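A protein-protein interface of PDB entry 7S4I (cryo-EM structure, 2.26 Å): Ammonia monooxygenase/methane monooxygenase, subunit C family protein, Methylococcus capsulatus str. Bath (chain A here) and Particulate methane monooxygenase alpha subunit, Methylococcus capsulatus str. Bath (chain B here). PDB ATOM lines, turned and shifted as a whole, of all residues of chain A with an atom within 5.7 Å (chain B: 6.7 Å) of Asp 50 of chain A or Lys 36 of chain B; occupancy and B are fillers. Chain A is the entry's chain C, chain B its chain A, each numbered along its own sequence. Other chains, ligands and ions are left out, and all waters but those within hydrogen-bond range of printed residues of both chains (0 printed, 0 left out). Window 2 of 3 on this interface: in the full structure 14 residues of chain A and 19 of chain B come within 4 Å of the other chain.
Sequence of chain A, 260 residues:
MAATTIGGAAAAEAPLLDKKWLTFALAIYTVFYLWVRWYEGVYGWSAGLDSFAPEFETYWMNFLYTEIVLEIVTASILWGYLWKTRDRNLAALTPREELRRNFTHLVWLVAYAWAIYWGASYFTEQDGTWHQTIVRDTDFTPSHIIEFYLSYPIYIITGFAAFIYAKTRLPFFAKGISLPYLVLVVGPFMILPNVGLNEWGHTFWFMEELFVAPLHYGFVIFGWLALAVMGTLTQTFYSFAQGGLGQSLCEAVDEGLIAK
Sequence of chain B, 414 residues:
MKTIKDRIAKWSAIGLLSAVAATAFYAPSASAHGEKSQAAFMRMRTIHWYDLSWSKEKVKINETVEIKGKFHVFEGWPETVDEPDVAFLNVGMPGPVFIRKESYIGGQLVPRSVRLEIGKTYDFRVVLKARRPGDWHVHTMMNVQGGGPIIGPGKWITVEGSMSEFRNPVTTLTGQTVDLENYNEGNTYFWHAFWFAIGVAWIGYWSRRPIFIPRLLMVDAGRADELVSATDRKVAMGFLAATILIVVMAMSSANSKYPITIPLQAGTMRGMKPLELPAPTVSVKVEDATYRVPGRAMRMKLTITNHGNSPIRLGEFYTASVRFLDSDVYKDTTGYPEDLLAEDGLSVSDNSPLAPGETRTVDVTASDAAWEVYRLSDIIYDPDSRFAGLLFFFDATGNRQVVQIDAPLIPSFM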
ATOM      1  N   GLY A  48       0.388  -9.103   5.097  1.00  0.00           N
ATOM      2  CA  GLY A  48       1.391  -8.937   6.130  1.00  0.00           C
ATOM      3  C   GLY A  48       2.497  -7.968   5.762  1.00  0.00           C
ATOM      4  O   GLY A  48       3.343  -7.644   6.599  1.00  0.00           O
ATOM      5  N   LEU A  49       2.499  -7.485   4.519  1.00  0.00           N
ATOM      6  CA  LEU A  49       3.426  -6.423   4.138  1.00  0.00           C
ATOM      7  C   LEU A  49       2.797  -5.043   4.311  1.00  0.00           C
ATOM      8  O   LEU A  49       3.447  -4.106   4.788  1.00  0.00           O
ATOM      9  CB  LEU A  49       3.896  -6.626   2.695  1.00  0.00           C
ATOM     10  CG  LEU A  49       5.105  -7.542   2.496  1.00  0.00           C
ATOM     11  CD1 LEU A  49       5.830  -7.195   1.209  1.00  0.00           C
ATOM     12  CD2 LEU A  49       6.050  -7.447   3.681  1.00  0.00           C
ATOM     13  N   ASP A  50       1.531  -4.898   3.923  1.00  0.00           N
ATOM     14  CA  ASP A  50       0.840  -3.618   4.017  1.00  0.00           C
ATOM     15  C   ASP A  50      -0.042  -3.608   5.260  1.00  0.00           C
ATOM     16  O   ASP A  50      -1.033  -4.342   5.330  1.00  0.00           O
ATOM     17  CB  ASP A  50       0.009  -3.371   2.759  1.00  0.00           C
ATOM     18  CG  ASP A  50      -0.737  -2.050   2.798  1.00  0.00           C
ATOM     19  OD1 ASP A  50      -0.363  -1.169   3.600  1.00  0.00           O
ATOM     20  OD2 ASP A  50      -1.695  -1.886   2.013  1.00  0.00           O
ATOM     21  N   SER A  51       0.307  -2.766   6.231  1.00  0.00           N
ATOM     22  CA  SER A  51      -0.392  -2.730   7.509  1.00  0.00           C
ATOM     23  C   SER A  51      -1.764  -2.071   7.429  1.00  0.00           C
ATOM     24  O   SER A  51      -2.527  -2.156   8.397  1.00  0.00           O
ATOM     25  CB  SER A  51       0.462  -2.008   8.552  1.00  0.00           C
ATOM     26  OG  SER A  51       0.437  -0.606   8.351  1.00  0.00           O
ATOM     27  N   PHE A  52      -2.097  -1.421   6.317  1.00  0.00           N
ATOM     28  CA  PHE A  52      -3.407  -0.811   6.139  1.00  0.00           C
ATOM     29  C   PHE A  52      -4.291  -1.581   5.170  1.00  0.00           C
ATOM     30  O   PHE A  52      -5.409  -1.138   4.887  1.00  0.00           O
ATOM     31  CB  PHE A  52      -3.254   0.641   5.673  1.00  0.00           C
ATOM     32  CG  PHE A  52      -2.838   1.582   6.766  1.00  0.00           C
ATOM     33  CD1 PHE A  52      -3.754   2.019   7.707  1.00  0.00           C
ATOM     34  CD2 PHE A  52      -1.529   2.022   6.860  1.00  0.00           C
ATOM     35  CE1 PHE A  52      -3.374   2.880   8.716  1.00  0.00           C
ATOM     36  CE2 PHE A  52      -1.144   2.883   7.867  1.00  0.00           C
ATOM     37  CZ  PHE A  52      -2.067   3.314   8.796  1.00  0.00           C
ATOM     38  N   ALA A  53      -3.825  -2.714   4.657  1.00  0.00           N
ATOM     39  CA  ALA A  53      -4.647  -3.562   3.813  1.00  0.00           C
ATOM     40  C   ALA A  53      -5.653  -4.334   4.659  1.00  0.00           C
ATOM     41  O   ALA A  53      -5.377  -4.676   5.811  1.00  0.00           O
ATOM     42  CB  ALA A  53      -3.766  -4.525   3.026  1.00  0.00           C
ATOM     43  N   PHE A  56      -4.383  -7.674   6.095  1.00  0.00           N
ATOM     44  CA  PHE A  56      -3.527  -7.561   7.267  1.00  0.00           C
ATOM     45  C   PHE A  56      -4.333  -7.643   8.552  1.00  0.00           C
ATOM     46  O   PHE A  56      -3.915  -8.318   9.494  1.00  0.00           O
ATOM     47  CB  PHE A  56      -2.736  -6.253   7.224  1.00  0.00           C
ATOM     48  CG  PHE A  56      -1.802  -6.066   8.388  1.00  0.00           C
ATOM     49  CD1 PHE A  56      -0.510  -6.561   8.339  1.00  0.00           C
ATOM     50  CD2 PHE A  56      -2.214  -5.397   9.529  1.00  0.00           C
ATOM     51  CE1 PHE A  56       0.353  -6.389   9.405  1.00  0.00           C
ATOM     52  CE2 PHE A  56      -1.355  -5.224  10.596  1.00  0.00           C
ATOM     53  CZ  PHE A  56      -0.072  -5.721  10.534  1.00  0.00           C
ATOM     54  N   ASP A 137       6.046  -0.831   8.708  1.00  0.00           N
ATOM     55  CA  ASP A 137       4.852  -0.054   8.420  1.00  0.00           C
ATOM     56  C   ASP A 137       4.062   0.329   9.659  1.00  0.00           C
ATOM     57  O   ASP A 137       3.142   1.149   9.557  1.00  0.00           O
ATOM     58  CB  ASP A 137       3.938  -0.835   7.465  1.00  0.00           C
ATOM     59  CG  ASP A 137       3.482  -0.008   6.288  1.00  0.00           C
ATOM     60  OD1 ASP A 137       4.130   1.019   6.001  1.00  0.00           O
ATOM     61  OD2 ASP A 137       2.476  -0.382   5.651  1.00  0.00           O
ATOM     62  N   HIS B  33       5.362  -0.475  -0.019  1.00  0.00           N
ATOM     63  CA  HIS B  33       4.387  -1.199   0.791  1.00  0.00           C
ATOM     64  C   HIS B  33       4.612  -0.577   2.160  1.00  0.00           C
ATOM     65  O   HIS B  33       3.756  -0.753   3.043  1.00  0.00           O
ATOM     66  CB  HIS B  33       4.634  -2.726   0.841  1.00  0.00           C
ATOM     67  CG  HIS B  33       3.803  -3.548  -0.097  1.00  0.00           C
ATOM     68  ND1 HIS B  33       3.511  -3.077  -1.348  1.00  0.00           N
ATOM     69  CD2 HIS B  33       3.231  -4.787  -0.014  1.00  0.00           C
ATOM     70  CE1 HIS B  33       2.756  -3.951  -1.979  1.00  0.00           C
ATOM     71  NE2 HIS B  33       2.613  -5.019  -1.218  1.00  0.00           N
ATOM     72  N   GLY B  34       5.738   0.140   2.295  1.00  0.00           N
ATOM     73  CA  GLY B  34       6.082   0.820   3.557  1.00  0.00           C
ATOM     74  C   GLY B  34       5.602   2.259   3.583  1.00  0.00           C
ATOM     75  O   GLY B  34       5.956   2.972   4.534  1.00  0.00           O
ATOM     76  N   GLU B  35       4.923   2.729   2.536  1.00  0.00           N
ATOM     77  CA  GLU B  35       4.340   4.100   2.622  1.00  0.00           C
ATOM     78  C   GLU B  35       2.863   3.942   3.024  1.00  0.00           C
ATOM     79  O   GLU B  35       2.512   2.825   3.477  1.00  0.00           O
ATOM     80  CB  GLU B  35       4.651   4.928   1.366  1.00  0.00           C
ATOM     81  CG  GLU B  35       3.586   4.899   0.291  1.00  0.00           C
ATOM     82  CD  GLU B  35       3.329   3.508  -0.245  1.00  0.00           C
ATOM     83  OE1 GLU B  35       4.169   3.011  -1.014  1.00  0.00           O
ATOM     84  OE2 GLU B  35       2.305   2.922   0.137  1.00  0.00           O
ATOM     85  N   LYS B  36       2.045   4.995   2.908  1.00  0.00           N
ATOM     86  CA  LYS B  36       0.633   4.956   3.397  1.00  0.00           C
ATOM     87  C   LYS B  36       0.650   4.951   4.930  1.00  0.00           C
ATOM     88  O   LYS B  36      -0.438   4.981   5.510  1.00  0.00           O
ATOM     89  CB  LYS B  36      -0.147   3.740   2.881  1.00  0.00           C
ATOM     90  CG  LYS B  36      -0.640   3.820   1.446  1.00  0.00           C
ATOM     91  CD  LYS B  36      -0.764   2.462   0.793  1.00  0.00           C
ATOM     92  CE  LYS B  36      -2.127   2.212   0.187  1.00  0.00           C
ATOM     93  NZ  LYS B  36      -2.937   1.303   1.032  1.00  0.00           N
ATOM     94  N   SER B  37       1.834   4.895   5.549  1.00  0.00           N
ATOM     95  CA  SER B  37       1.980   4.906   7.025  1.00  0.00           C
ATOM     96  C   SER B  37       2.818   6.121   7.418  1.00  0.00           C
ATOM     97  O   SER B  37       2.623   6.623   8.533  1.00  0.00           O
ATOM     98  CB  SER B  37       2.607   3.634   7.518  1.00  0.00           C
ATOM     99  OG  SER B  37       1.809   2.516   7.166  1.00  0.00           O
ATOM    100  N   GLN B  38       3.713   6.578   6.533  1.00  0.00           N
ATOM    101  CA  GLN B  38       4.460   7.787   6.827  1.00  0.00           C
ATOM    102  C   GLN B  38       3.545   9.006   6.791  1.00  0.00           C
ATOM    103  O   GLN B  38       2.455   8.985   6.212  1.00  0.00           O
ATOM    104  CB  GLN B  38       5.610   7.960   5.836  1.00  0.00           C
ATOM    105  CG  GLN B  38       6.226   6.657   5.376  1.00  0.00           C
ATOM    106  CD  GLN B  38       7.375   6.869   4.413  1.00  0.00           C
ATOM    107  OE1 GLN B  38       7.191   6.847   3.198  1.00  0.00           O
ATOM    108  NE2 GLN B  38       8.569   7.075   4.954  1.00  0.00           N
ATOM    109  N   ALA B  39       4.002  10.075   7.436  1.00  0.00           N
ATOM    110  CA  ALA B  39       3.224  11.303   7.507  1.00  0.00           C
ATOM    111  C   ALA B  39       2.948  11.847   6.111  1.00  0.00           C
ATOM    112  O   ALA B  39       3.828  11.853   5.243  1.00  0.00           O
ATOM    113  CB  ALA B  39       3.959  12.343   8.350  1.00  0.00           C
ATOM    114  N   ARG B  43       5.601  12.849   3.134  1.00  0.00           N
ATOM    115  CA  ARG B  43       5.589  12.243   1.809  1.00  0.00           C
ATOM    116  C   ARG B  43       5.395  13.292   0.723  1.00  0.00           C
ATOM    117  O   ARG B  43       5.926  13.147  -0.384  1.00  0.00           O
ATOM    118  CB  ARG B  43       4.495  11.180   1.721  1.00  0.00           C
ATOM    119  CG  ARG B  43       4.868   9.857   2.357  1.00  0.00           C
ATOM    120  CD  ARG B  43       3.803   8.811   2.100  1.00  0.00           C
ATOM    121  NE  ARG B  43       2.682   8.947   3.020  1.00  0.00           N
ATOM    122  CZ  ARG B  43       1.410   8.811   2.675  1.00  0.00           C
ATOM    123  NH1 ARG B  43       1.058   8.518   1.434  1.00  0.00           N
ATOM    124  NH2 ARG B  43       0.467   8.969   3.599  1.00  0.00           N
ATOM    125  N   ASP B 339      -3.506   2.310  -9.185  1.00  0.00           N
ATOM    126  CA  ASP B 339      -3.966   2.794  -7.889  1.00  0.00           C
ATOM    127  C   ASP B 339      -3.354   4.140  -7.522  1.00  0.00           C
ATOM    128  O   ASP B 339      -3.877   4.822  -6.636  1.00  0.00           O
ATOM    129  CB  ASP B 339      -3.661   1.756  -6.807  1.00  0.00           C
ATOM    130  CG  ASP B 339      -2.196   1.717  -6.431  1.00  0.00           C
ATOM    131  OD1 ASP B 339      -1.343   1.805  -7.337  1.00  0.00           O
ATOM    132  OD2 ASP B 339      -1.895   1.588  -5.226  1.00  0.00           O
ATOM    133  N   GLU B 372      -7.566   8.929  -0.157  1.00  0.00           N
ATOM    134  CA  GLU B 372      -7.864   8.242   1.090  1.00  0.00           C
ATOM    135  C   GLU B 372      -7.192   6.885   1.209  1.00  0.00           C
ATOM    136  O   GLU B 372      -6.877   6.468   2.325  1.00  0.00           O
ATOM    137  CB  GLU B 372      -9.381   8.060   1.251  1.00  0.00           C
ATOM    138  CG  GLU B 372     -10.067   9.217   1.953  1.00  0.00           C
ATOM    139  CD  GLU B 372     -11.528   8.941   2.247  1.00  0.00           C
ATOM    140  OE1 GLU B 372     -12.117   8.072   1.570  1.00  0.00           O
ATOM    141  OE2 GLU B 372     -12.089   9.596   3.150  1.00  0.00           O
ATOM    142  N   VAL B 373      -6.971   6.183   0.094  1.00  0.00           N
ATOM    143  CA  VAL B 373      -6.313   4.883   0.150  1.00  0.00           C
ATOM    144  C   VAL B 373      -4.875   5.020   0.634  1.00  0.00           C
ATOM    145  O   VAL B 373      -4.432   4.259   1.504  1.00  0.00           O
ATOM    146  CB  VAL B 373      -6.385   4.194  -1.225  1.00  0.00           C
ATOM    147  CG1 VAL B 373      -5.362   3.077  -1.319  1.00  0.00           C
ATOM    148  CG2 VAL B 373      -7.787   3.661  -1.475  1.00  0.00           C
ATOM    149  N   TYR B 374      -4.127   5.986   0.102  1.00  0.00           N
ATOM    150  CA  TYR B 374      -2.756   6.235   0.519  1.00  0.00           C
ATOM    151  C   TYR B 374      -2.679   7.199   1.695  1.00  0.00           C
ATOM    152  O   TYR B 374      -1.599   7.716   1.996  1.00  0.00           O
ATOM    153  CB  TYR B 374      -1.935   6.749  -0.663  1.00  0.00           C
ATOM    154  CG  TYR B 374      -1.442   5.632  -1.549  1.00  0.00           C
ATOM    155  CD1 TYR B 374      -2.298   4.998  -2.438  1.00  0.00           C
ATOM    156  CD2 TYR B 374      -0.124   5.201  -1.488  1.00  0.00           C
ATOM    157  CE1 TYR B 374      -1.856   3.969  -3.242  1.00  0.00           C
ATOM    158  CE2 TYR B 374       0.327   4.174  -2.290  1.00  0.00           C
ATOM    159  CZ  TYR B 374      -0.543   3.561  -3.165  1.00  0.00           C
ATOM    160  OH  TYR B 374      -0.095   2.538  -3.967  1.00  0.00           O
ATOM    161  N   ARG B 375      -3.817   7.396   2.372  1.00  0.00           N
ATOM    162  CA  ARG B 375      -3.865   8.224   3.610  1.00  0.00           C
ATOM    163  C   ARG B 375      -3.249   9.611   3.404  1.00  0.00           C
ATOM    164  O   ARG B 375      -2.509  10.065   4.302  1.00  0.00           O
ATOM    165  CB  ARG B 375      -3.220   7.448   4.764  1.00  0.00           C
ATOM    166  CG  ARG B 375      -4.044   6.256   5.231  1.00  0.00           C
ATOM    167  CD  ARG B 375      -3.894   6.064   6.724  1.00  0.00           C
ATOM    168  NE  ARG B 375      -2.478   6.169   7.032  1.00  0.00           N
ATOM    169  CZ  ARG B 375      -1.953   6.715   8.120  1.00  0.00           C
ATOM    170  NH1 ARG B 375      -2.726   7.212   9.070  1.00  0.00           N
ATOM    171  NH2 ARG B 375      -0.642   6.740   8.252  1.00  0.00           N
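Of chain B, only Lys 36 (3.6 Å) comes within 4 Å of Asp 50 of chain A. Of the printed residues of chain B, Ser 51 of chain A touches Ser 37 (3.6 Å). Printed residues of chain A within 4 Å of His 33 of chain B: Leu 49 (3.3 Å) and Asp 137 (2.9 Å). Of the printed residues of chain A, Gly 34 of chain B touches Asp 137 (3.0 Å). Of chain A, only Asp 50 and Phe 52 come within 4 Å of Lys 36 of chain B. Of the printed residues of chain A, Ser 37 of chain B touches Ser 51 (3.6 Å), Phe 52 (3.1 Å) and Asp 137 (3.0 Å). Gln 38 of chain B touches none of the printed residues of chain A. Printed residues of chain A within 4 Å of Arg 375 of chain B: Phe 52. The nearest residue of chain B that does not touch Asp 50 of chain A is His 33 of chain B (4.2 Å). The nearest printed residue of chain A that does not touch Gly 34 of chain B is Leu 49 of chain A (5.4 Å).
Printed residues of chain B that touch a printed residue of chain A: His 33, Gly 34, Glu 35, Lys 36, Ser 37 and Arg 375. Hydrophobic or aromatic side chains of chain B that line the printed part of chain A: His 33. Along chain B the printed residues that touch a printed residue of chain A span positions 33 to 375. Of the 8 printed residues of chain A, 5 touch a printed residue of chain B. Printed residues of chain A that touch a printed residue of chain B: Leu 49, Asp 50, Ser 51, Phe 52 and Asp 137. Hydrophobic or aromatic side chains of chain A within 4 Å of the printed part of chain B: Leu 49 and Phe 52. Along chain A the printed residues that touch a printed residue of chain B span positions 49 to 137.
Leu 49 of chain A touches His 33 of chain B (CB to CD2, 3.3 Å). Ser 51 of chain A touches Ser 37 of chain B. O of Lys 36 of chain B touches CE2 of Phe 52 of chain A (3.2 Å). OG of Ser 37 of chain B touches CE2 of Phe 52 of chain A, at 3.1 Å. Phe 52 of chain A touches Arg 375 of chain B. Glu 35 of chain B touches Asp 137 of chain A (O to OD1, 3.5 Å).
The backbone carbonyl oxygen (O) of Lys 36 of chain B sits at hydrogen-bond distance from the guanidinium group (NE) of Arg 375 of chain B (2.8 Å). The backbone carbonyl oxygen (O) of Ser 37 of chain B is in hydrogen-bond range of the guanidinium group (NH2) of Arg 375 of chain B (3.3 Å). NH2 of Arg 43 of chain B lies within hydrogen-bond range of O of Arg 375 of chain B (3.2 Å). The side-chain carboxylate (OD1) of Asp 50 of chain A lies close to the backbone NH (N) of Phe 52 of chain A, at 3.2 Å. The side-chain carboxylate of Asp 50 of chain A lies within hydrogen-bond range of the backbone NH of Ala 53 of chain A, 3.5 Å away. The side-chain carboxylate (OD2) of Asp 137 of chain A sits at hydrogen-bond distance from the backbone NH (N) of Ser 51 of chain A, at 3.3 Å.
The side-chain carboxylate of Asp 50 of chain A is in salt-bridge range of the side-chain amino group of Lys 36 of chain B (3.6 Å). The side-chain hydroxyl of Ser 37 of chain B is in hydrogen-bond range of the side-chain carboxylate of Asp 137 of chain A (3.0 Å). O of His 33 of chain B sits close to OD2 of Asp 137 of chain A, 2.9 Å away. O of Gly 34 of chain B sits close to OD1 of Asp 137 of chain A, 3.0 Å away.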
